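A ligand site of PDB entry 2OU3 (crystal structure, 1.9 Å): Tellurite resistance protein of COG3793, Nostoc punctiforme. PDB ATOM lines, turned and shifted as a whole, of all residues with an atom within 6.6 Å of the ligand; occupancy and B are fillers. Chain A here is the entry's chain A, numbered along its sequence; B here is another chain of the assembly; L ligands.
A nitrogen (N1) of the ligand is in hydrogen-bond range of the side-chain carboxylate (OD2) of Asp 96 (2.8 Å). O1 of the ligand sits at hydrogen-bond distance from OG of Ser 29.
N of Gln 89 lies within hydrogen-bond range of OG of Ser 87 (3.1 Å). The side-chain carboxylate (OD1) of Asp 96 is in hydrogen-bond range of the side-chain hydroxyl (OH) of Tyr 32 (2.5 Å). OD1 of Asp 28 lies within hydrogen-bond range of OG of Ser 87 (2.7 Å). OH of Tyr 161 of chain B sits at hydrogen-bond distance from OD2 of Asp 28 (2.4 Å). The backbone NH of Val 90 lies within hydrogen-bond range of the side-chain hydroxyl of Ser 87, at 3.1 Å. OG1 of Thr 25 sits at hydrogen-bond distance from N of Asp 28, 3.1 Å away. OG of Ser 100 sits at hydrogen-bond distance from O of Asp 96, at 3.5 Å. The side-chain hydroxyl (OH) of Tyr 32 sits at hydrogen-bond distance from the side-chain hydroxyl (OG) of Ser 100.
Phe 18 touches the ligand. Phe 20 touches the ligand. Pro 24 touches the ligand (CG to O1, 3.5 Å). Asp 28 touches the ligand. Tyr 32 touches the ligand. Trp 61 touches the ligand (CZ3 to C1, 3.3 Å). O of Gln 89 touches C8 of the ligand, 3.7 Å away. Val 90 touches the ligand (CG2 to C7, 3.9 Å). CB of Ala 93 touches C9 of the ligand, at 3.6 Å. Tyr 155 of chain B touches the ligand. Pro 160 of chain B touches the ligand. Tyr 161 of chain B touches the ligand (CE2 to C7, 3.9 Å). Hydrophobic or aromatic side chains that line the ligand: Phe 18, Phe 20, Pro 24, Tyr 32, Trp 61, Val 90, Ala 93, Pro 160 of chain B and Tyr 161 of chain B. 14 residues have an atom within 4 Å of the ligand: Phe 18, Phe 20, Pro 24, Asp 28, Ser 29, Tyr 32, Trp 61, Gln 89, Val 90, Ala 93, Asp 96, Tyr 155 of chain B, Pro 160 of chain B and Tyr 161 of chain B. The nearest printed residue that does not touch the ligand is Ile 14 (4.3 Å).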
ATOM      1  N   ILE A  14      17.606 -15.367  17.103  1.00  0.00           N
ATOM      2  CA  ILE A  14      16.717 -14.291  16.659  1.00  0.00           C
ATOM      3  C   ILE A  14      17.521 -13.248  15.918  1.00  0.00           C
ATOM      4  O   ILE A  14      17.141 -12.812  14.820  1.00  0.00           O
ATOM      5  CB  ILE A  14      15.971 -13.666  17.844  1.00  0.00           C
ATOM      6  CG1 ILE A  14      14.865 -14.580  18.278  1.00  0.00           C
ATOM      7  CG2 ILE A  14      15.428 -12.305  17.452  1.00  0.00           C
ATOM      8  CD1 ILE A  14      13.677 -14.688  17.234  1.00  0.00           C
ATOM      9  N   PHE A  18      16.808 -12.650  11.919  1.00  0.00           N
ATOM     10  CA  PHE A  18      15.983 -11.437  11.727  1.00  0.00           C
ATOM     11  C   PHE A  18      16.701 -10.110  11.950  1.00  0.00           C
ATOM     12  O   PHE A  18      16.148  -9.065  11.605  1.00  0.00           O
ATOM     13  CB  PHE A  18      14.721 -11.509  12.569  1.00  0.00           C
ATOM     14  CG  PHE A  18      13.962 -12.798  12.384  1.00  0.00           C
ATOM     15  CD1 PHE A  18      13.293 -13.040  11.201  1.00  0.00           C
ATOM     16  CD2 PHE A  18      14.060 -13.812  13.336  1.00  0.00           C
ATOM     17  CE1 PHE A  18      12.647 -14.239  10.998  1.00  0.00           C
ATOM     18  CE2 PHE A  18      13.388 -15.034  13.160  1.00  0.00           C
ATOM     19  CZ  PHE A  18      12.710 -15.256  11.979  1.00  0.00           C
ATOM     20  N   PHE A  20      17.370  -8.782  14.841  1.00  0.00           N
ATOM     21  CA  PHE A  20      16.775  -8.133  15.996  1.00  0.00           C
ATOM     22  C   PHE A  20      17.751  -8.131  17.146  1.00  0.00           C
ATOM     23  O   PHE A  20      18.521  -9.052  17.301  1.00  0.00           O
ATOM     24  CB  PHE A  20      15.509  -8.907  16.432  1.00  0.00           C
ATOM     25  CG  PHE A  20      14.357  -8.875  15.439  1.00  0.00           C
ATOM     26  CD1 PHE A  20      14.321  -8.001  14.355  1.00  0.00           C
ATOM     27  CD2 PHE A  20      13.284  -9.761  15.616  1.00  0.00           C
ATOM     28  CE1 PHE A  20      13.231  -7.988  13.451  1.00  0.00           C
ATOM     29  CE2 PHE A  20      12.191  -9.732  14.737  1.00  0.00           C
ATOM     30  CZ  PHE A  20      12.169  -8.852  13.671  1.00  0.00           C
ATOM     31  N   PRO A  24      11.652 -11.317  20.528  1.00  0.00           N
ATOM     32  CA  PRO A  24      10.218 -10.972  20.524  1.00  0.00           C
ATOM     33  C   PRO A  24       9.455 -11.700  21.631  1.00  0.00           C
ATOM     34  O   PRO A  24       9.838 -12.811  22.054  1.00  0.00           O
ATOM     35  CB  PRO A  24       9.740 -11.468  19.133  1.00  0.00           C
ATOM     36  CG  PRO A  24      10.985 -11.429  18.297  1.00  0.00           C
ATOM     37  CD  PRO A  24      12.065 -11.924  19.240  1.00  0.00           C
ATOM     38  N   THR A  25       8.362 -11.071  22.067  1.00  0.00           N
ATOM     39  CA  THR A  25       7.469 -11.704  23.022  1.00  0.00           C
ATOM     40  C   THR A  25       6.939 -12.979  22.412  1.00  0.00           C
ATOM     41  O   THR A  25       6.874 -13.098  21.160  1.00  0.00           O
ATOM     42  CB  THR A  25       6.295 -10.772  23.391  1.00  0.00           C
ATOM     43  OG1 THR A  25       5.585 -10.460  22.211  1.00  0.00           O
ATOM     44  CG2 THR A  25       6.816  -9.462  24.072  1.00  0.00           C
ATOM     45  N   ASP A  28       4.105 -12.112  20.097  1.00  0.00           N
ATOM     46  CA  ASP A  28       4.562 -11.674  18.774  1.00  0.00           C
ATOM     47  C   ASP A  28       5.066 -12.814  17.901  1.00  0.00           C
ATOM     48  O   ASP A  28       4.772 -12.842  16.709  1.00  0.00           O
ATOM     49  CB  ASP A  28       5.619 -10.571  18.870  1.00  0.00           C
ATOM     50  CG  ASP A  28       5.024  -9.158  19.006  1.00  0.00           C
ATOM     51  OD1 ASP A  28       3.785  -8.990  18.848  1.00  0.00           O
ATOM     52  OD2 ASP A  28       5.832  -8.198  19.227  1.00  0.00           O
ATOM     53  N   SER A  29       5.806 -13.755  18.485  1.00  0.00           N
ATOM     54  CA  SER A  29       6.235 -14.926  17.716  1.00  0.00           C
ATOM     55  C   SER A  29       5.018 -15.677  17.197  1.00  0.00           C
ATOM     56  O   SER A  29       4.974 -16.086  16.024  1.00  0.00           O
ATOM     57  CB  SER A  29       7.132 -15.869  18.544  1.00  0.00           C
ATOM     58  OG  SER A  29       8.403 -15.273  18.824  1.00  0.00           O
ATOM     59  N   SER A  30       4.015 -15.822  18.052  1.00  0.00           N
ATOM     60  CA  SER A  30       2.763 -16.487  17.696  1.00  0.00           C
ATOM     61  C   SER A  30       2.026 -15.797  16.535  1.00  0.00           C
ATOM     62  O   SER A  30       1.693 -16.428  15.529  1.00  0.00           O
ATOM     63  CB  SER A  30       1.841 -16.556  18.929  1.00  0.00           C
ATOM     64  OG  SER A  30       0.604 -17.190  18.644  1.00  0.00           O
ATOM     65  N   TYR A  32       3.226 -13.552  14.431  1.00  0.00           N
ATOM     66  CA  TYR A  32       4.091 -13.611  13.253  1.00  0.00           C
ATOM     67  C   TYR A  32       3.939 -14.946  12.520  1.00  0.00           C
ATOM     68  O   TYR A  32       3.720 -14.958  11.297  1.00  0.00           O
ATOM     69  CB  TYR A  32       5.542 -13.419  13.660  1.00  0.00           C
ATOM     70  CG  TYR A  32       6.565 -13.634  12.553  1.00  0.00           C
ATOM     71  CD1 TYR A  32       6.866 -12.620  11.659  1.00  0.00           C
ATOM     72  CD2 TYR A  32       7.221 -14.848  12.406  1.00  0.00           C
ATOM     73  CE1 TYR A  32       7.802 -12.806  10.645  1.00  0.00           C
ATOM     74  CE2 TYR A  32       8.144 -15.046  11.406  1.00  0.00           C
ATOM     75  CZ  TYR A  32       8.450 -14.036  10.535  1.00  0.00           C
ATOM     76  OH  TYR A  32       9.392 -14.252   9.561  1.00  0.00           O
ATOM     77  N   MET A  33       4.013 -16.048  13.249  1.00  0.00           N
ATOM     78  CA  MET A  33       3.905 -17.383  12.647  1.00  0.00           C
ATOM     79  C   MET A  33       2.526 -17.645  12.096  1.00  0.00           C
ATOM     80  O   MET A  33       2.390 -18.276  11.061  1.00  0.00           O
ATOM     81  CB  MET A  33       4.264 -18.496  13.627  1.00  0.00           C
ATOM     82  CG  MET A  33       5.737 -18.670  13.815  1.00  0.00           C
ATOM     83  SD  MET A  33       6.696 -18.965  12.147  1.00  0.00           S
ATOM     84  CE  MET A  33       5.524 -20.131  11.339  1.00  0.00           C
ATOM     85  N   TRP A  61      13.494 -20.891  17.832  1.00  0.00           N
ATOM     86  CA  TRP A  61      13.751 -19.588  18.500  1.00  0.00           C
ATOM     87  C   TRP A  61      13.635 -19.690  20.010  1.00  0.00           C
ATOM     88  O   TRP A  61      13.896 -18.717  20.729  1.00  0.00           O
ATOM     89  CB  TRP A  61      12.815 -18.474  18.056  1.00  0.00           C
ATOM     90  CG  TRP A  61      12.560 -18.456  16.592  1.00  0.00           C
ATOM     91  CD1 TRP A  61      13.422 -18.834  15.620  1.00  0.00           C
ATOM     92  CD2 TRP A  61      11.359 -18.035  15.935  1.00  0.00           C
ATOM     93  NE1 TRP A  61      12.834 -18.685  14.383  1.00  0.00           N
ATOM     94  CE2 TRP A  61      11.572 -18.189  14.557  1.00  0.00           C
ATOM     95  CE3 TRP A  61      10.120 -17.533  16.377  1.00  0.00           C
ATOM     96  CZ2 TRP A  61      10.594 -17.884  13.608  1.00  0.00           C
ATOM     97  CZ3 TRP A  61       9.165 -17.244  15.445  1.00  0.00           C
ATOM     98  CH2 TRP A  61       9.397 -17.420  14.080  1.00  0.00           C
ATOM     99  N   VAL A  63      10.781 -20.234  21.719  1.00  0.00           N
ATOM    100  CA  VAL A  63       9.439 -19.814  22.175  1.00  0.00           C
ATOM    101  C   VAL A  63       8.878 -20.759  23.256  1.00  0.00           C
ATOM    102  O   VAL A  63       9.240 -21.933  23.341  1.00  0.00           O
ATOM    103  CB  VAL A  63       8.410 -19.693  21.034  1.00  0.00           C
ATOM    104  CG1 VAL A  63       8.843 -18.640  20.061  1.00  0.00           C
ATOM    105  CG2 VAL A  63       8.098 -21.062  20.336  1.00  0.00           C
ATOM    106  N   SER A  87      -0.659  -6.969  16.238  1.00  0.00           N
ATOM    107  CA  SER A  87       0.599  -6.503  16.824  1.00  0.00           C
ATOM    108  C   SER A  87       1.257  -5.370  16.056  1.00  0.00           C
ATOM    109  O   SER A  87       1.469  -5.493  14.842  1.00  0.00           O
ATOM    110  CB  SER A  87       1.568  -7.673  16.821  1.00  0.00           C
ATOM    111  OG  SER A  87       2.895  -7.231  17.072  1.00  0.00           O
ATOM    112  N   GLN A  89       4.329  -4.687  16.048  1.00  0.00           N
ATOM    113  CA  GLN A  89       5.611  -5.247  15.598  1.00  0.00           C
ATOM    114  C   GLN A  89       5.401  -6.118  14.380  1.00  0.00           C
ATOM    115  O   GLN A  89       6.083  -5.980  13.376  1.00  0.00           O
ATOM    116  CB  GLN A  89       6.293  -6.070  16.701  1.00  0.00           C
ATOM    117  CG  GLN A  89       6.812  -5.239  17.905  1.00  0.00           C
ATOM    118  CD  GLN A  89       5.694  -4.697  18.778  1.00  0.00           C
ATOM    119  OE1 GLN A  89       4.888  -5.463  19.344  1.00  0.00           O
ATOM    120  NE2 GLN A  89       5.641  -3.368  18.897  1.00  0.00           N
ATOM    121  N   VAL A  90       4.417  -7.004  14.438  1.00  0.00           N
ATOM    122  CA  VAL A  90       4.123  -7.821  13.265  1.00  0.00           C
ATOM    123  C   VAL A  90       3.658  -6.945  12.067  1.00  0.00           C
ATOM    124  O   VAL A  90       3.883  -7.267  10.907  1.00  0.00           O
ATOM    125  CB  VAL A  90       3.147  -8.992  13.577  1.00  0.00           C
ATOM    126  CG1 VAL A  90       2.880  -9.874  12.310  1.00  0.00           C
ATOM    127  CG2 VAL A  90       3.743  -9.833  14.683  1.00  0.00           C
ATOM    128  N   SER A  91       3.039  -5.821  12.386  1.00  0.00           N
ATOM    129  CA  SER A  91       2.559  -4.906  11.380  1.00  0.00           C
ATOM    130  C   SER A  91       3.709  -4.113  10.710  1.00  0.00           C
ATOM    131  O   SER A  91       3.440  -3.290   9.882  1.00  0.00           O
ATOM    132  CB  SER A  91       1.495  -3.972  11.975  1.00  0.00           C
ATOM    133  OG  SER A  91       0.278  -4.668  12.240  1.00  0.00           O
ATOM    134  N   MET A  92       4.964  -4.367  11.087  1.00  0.00           N
ATOM    135  CA  MET A  92       6.151  -3.851  10.405  1.00  0.00           C
ATOM    136  C   MET A  92       6.875  -4.948   9.591  1.00  0.00           C
ATOM    137  O   MET A  92       7.885  -4.681   8.927  1.00  0.00           O
ATOM    138  CB  MET A  92       7.136  -3.278  11.439  1.00  0.00           C
ATOM    139  CG  MET A  92       6.549  -2.221  12.278  1.00  0.00           C
ATOM    140  SD  MET A  92       7.681  -1.624  13.738  1.00  0.00           S
ATOM    141  CE  MET A  92       8.935  -1.428  12.745  1.00  0.00           C
ATOM    142  N   ALA A  93       6.352  -6.166   9.658  1.00  0.00           N
ATOM    143  CA  ALA A  93       7.079  -7.373   9.308  1.00  0.00           C
ATOM    144  C   ALA A  93       6.653  -7.952   7.963  1.00  0.00           C
ATOM    145  O   ALA A  93       6.910  -9.121   7.681  1.00  0.00           O
ATOM    146  CB  ALA A  93       6.875  -8.415  10.427  1.00  0.00           C
ATOM    147  N   ASP A  96       9.315  -9.717   5.810  1.00  0.00           N
ATOM    148  CA  ASP A  96       9.821 -10.788   6.641  1.00  0.00           C
ATOM    149  C   ASP A  96       8.813 -11.958   6.615  1.00  0.00           C
ATOM    150  O   ASP A  96       9.178 -13.103   6.385  1.00  0.00           O
ATOM    151  CB  ASP A  96      10.022 -10.164   8.025  1.00  0.00           C
ATOM    152  CG  ASP A  96      10.589 -11.107   9.082  1.00  0.00           C
ATOM    153  OD1 ASP A  96      10.812 -12.323   8.829  1.00  0.00           O
ATOM    154  OD2 ASP A  96      10.847 -10.551  10.194  1.00  0.00           O
ATOM    155  N   ILE A  97       7.543 -11.648   6.805  1.00  0.00           N
ATOM    156  CA  ILE A  97       6.507 -12.654   6.777  1.00  0.00           C
ATOM    157  C   ILE A  97       6.541 -13.366   5.391  1.00  0.00           C
ATOM    158  O   ILE A  97       6.454 -14.588   5.306  1.00  0.00           O
ATOM    159  CB  ILE A  97       5.070 -12.002   6.973  1.00  0.00           C
ATOM    160  CG1 ILE A  97       4.855 -11.546   8.439  1.00  0.00           C
ATOM    161  CG2 ILE A  97       3.948 -12.966   6.517  1.00  0.00           C
ATOM    162  CD1 ILE A  97       3.758 -10.436   8.618  1.00  0.00           C
ATOM    163  N   SER A 100       9.544 -15.780   4.888  1.00  0.00           N
ATOM    164  CA  SER A 100       9.303 -17.031   5.625  1.00  0.00           C
ATOM    165  C   SER A 100       8.231 -17.883   4.939  1.00  0.00           C
ATOM    166  O   SER A 100       8.370 -19.083   4.845  1.00  0.00           O
ATOM    167  CB  SER A 100       8.895 -16.732   7.069  1.00  0.00           C
ATOM    168  OG  SER A 100       9.997 -16.198   7.797  1.00  0.00           O
ATOM    169  N   TYR B 155      14.197  -5.178   6.314  1.00  0.00           N
ATOM    170  CA  TYR B 155      14.048  -4.005   7.201  1.00  0.00           C
ATOM    171  C   TYR B 155      14.994  -2.878   6.765  1.00  0.00           C
ATOM    172  O   TYR B 155      15.997  -2.588   7.421  1.00  0.00           O
ATOM    173  CB  TYR B 155      14.269  -4.387   8.680  1.00  0.00           C
ATOM    174  CG  TYR B 155      13.238  -5.381   9.193  1.00  0.00           C
ATOM    175  CD1 TYR B 155      11.923  -4.984   9.464  1.00  0.00           C
ATOM    176  CD2 TYR B 155      13.584  -6.694   9.414  1.00  0.00           C
ATOM    177  CE1 TYR B 155      10.970  -5.894   9.898  1.00  0.00           C
ATOM    178  CE2 TYR B 155      12.603  -7.643   9.881  1.00  0.00           C
ATOM    179  CZ  TYR B 155      11.300  -7.217  10.086  1.00  0.00           C
ATOM    180  OH  TYR B 155      10.329  -8.067  10.539  1.00  0.00           O
ATOM    181  N   PRO B 160      11.216  -3.873  13.972  1.00  0.00           N
ATOM    182  CA  PRO B 160      10.382  -3.988  15.164  1.00  0.00           C
ATOM    183  C   PRO B 160      11.119  -4.339  16.445  1.00  0.00           C
ATOM    184  O   PRO B 160      10.697  -3.948  17.539  1.00  0.00           O
ATOM    185  CB  PRO B 160       9.382  -5.096  14.811  1.00  0.00           C
ATOM    186  CG  PRO B 160       9.991  -5.847  13.737  1.00  0.00           C
ATOM    187  CD  PRO B 160      10.853  -4.895  12.975  1.00  0.00           C
ATOM    188  N   TYR B 161      12.207  -5.076  16.314  1.00  0.00           N
ATOM    189  CA  TYR B 161      12.974  -5.483  17.460  1.00  0.00           C
ATOM    190  C   TYR B 161      14.459  -5.375  17.134  1.00  0.00           C
ATOM    191  O   TYR B 161      15.327  -5.588  17.960  1.00  0.00           O
ATOM    192  CB  TYR B 161      12.641  -6.924  17.762  1.00  0.00           C
ATOM    193  CG  TYR B 161      11.347  -7.188  18.496  1.00  0.00           C
ATOM    194  CD1 TYR B 161      11.240  -6.981  19.855  1.00  0.00           C
ATOM    195  CD2 TYR B 161      10.240  -7.728  17.832  1.00  0.00           C
ATOM    196  CE1 TYR B 161      10.089  -7.305  20.545  1.00  0.00           C
ATOM    197  CE2 TYR B 161       9.082  -8.065  18.505  1.00  0.00           C
ATOM    198  CZ  TYR B 161       8.999  -7.832  19.859  1.00  0.00           C
ATOM    199  OH  TYR B 161       7.854  -8.191  20.576  1.00  0.00           O
ATOM    200  OXT TYR B 161      14.791  -5.035  16.001  1.00  0.00           O
HETATM  201  O1  LIG L   1       9.148 -13.835  16.530  1.00  0.00           O
HETATM  202  C1  LIG L   1       9.787 -13.963  15.484  1.00  0.00           C
HETATM  203  C2  LIG L   1       9.734 -12.845  14.511  1.00  0.00           C
HETATM  204  C3  LIG L   1      10.430 -12.816  13.340  1.00  0.00           C
HETATM  205  N1  LIG L   1      10.148 -11.623  12.714  1.00  0.00           N
HETATM  206  C4  LIG L   1       9.289 -10.872  13.437  1.00  0.00           C
HETATM  207  C5  LIG L   1       8.958 -11.611  14.669  1.00  0.00           C
HETATM  208  C6  LIG L   1       8.108 -11.055  15.635  1.00  0.00           C
HETATM  209  C7  LIG L   1       7.560  -9.819  15.388  1.00  0.00           C
HETATM  210  C8  LIG L   1       7.867  -9.092  14.232  1.00  0.00           C
HETATM  211  C9  LIG L   1       8.734  -9.626  13.278  1.00  0.00           C
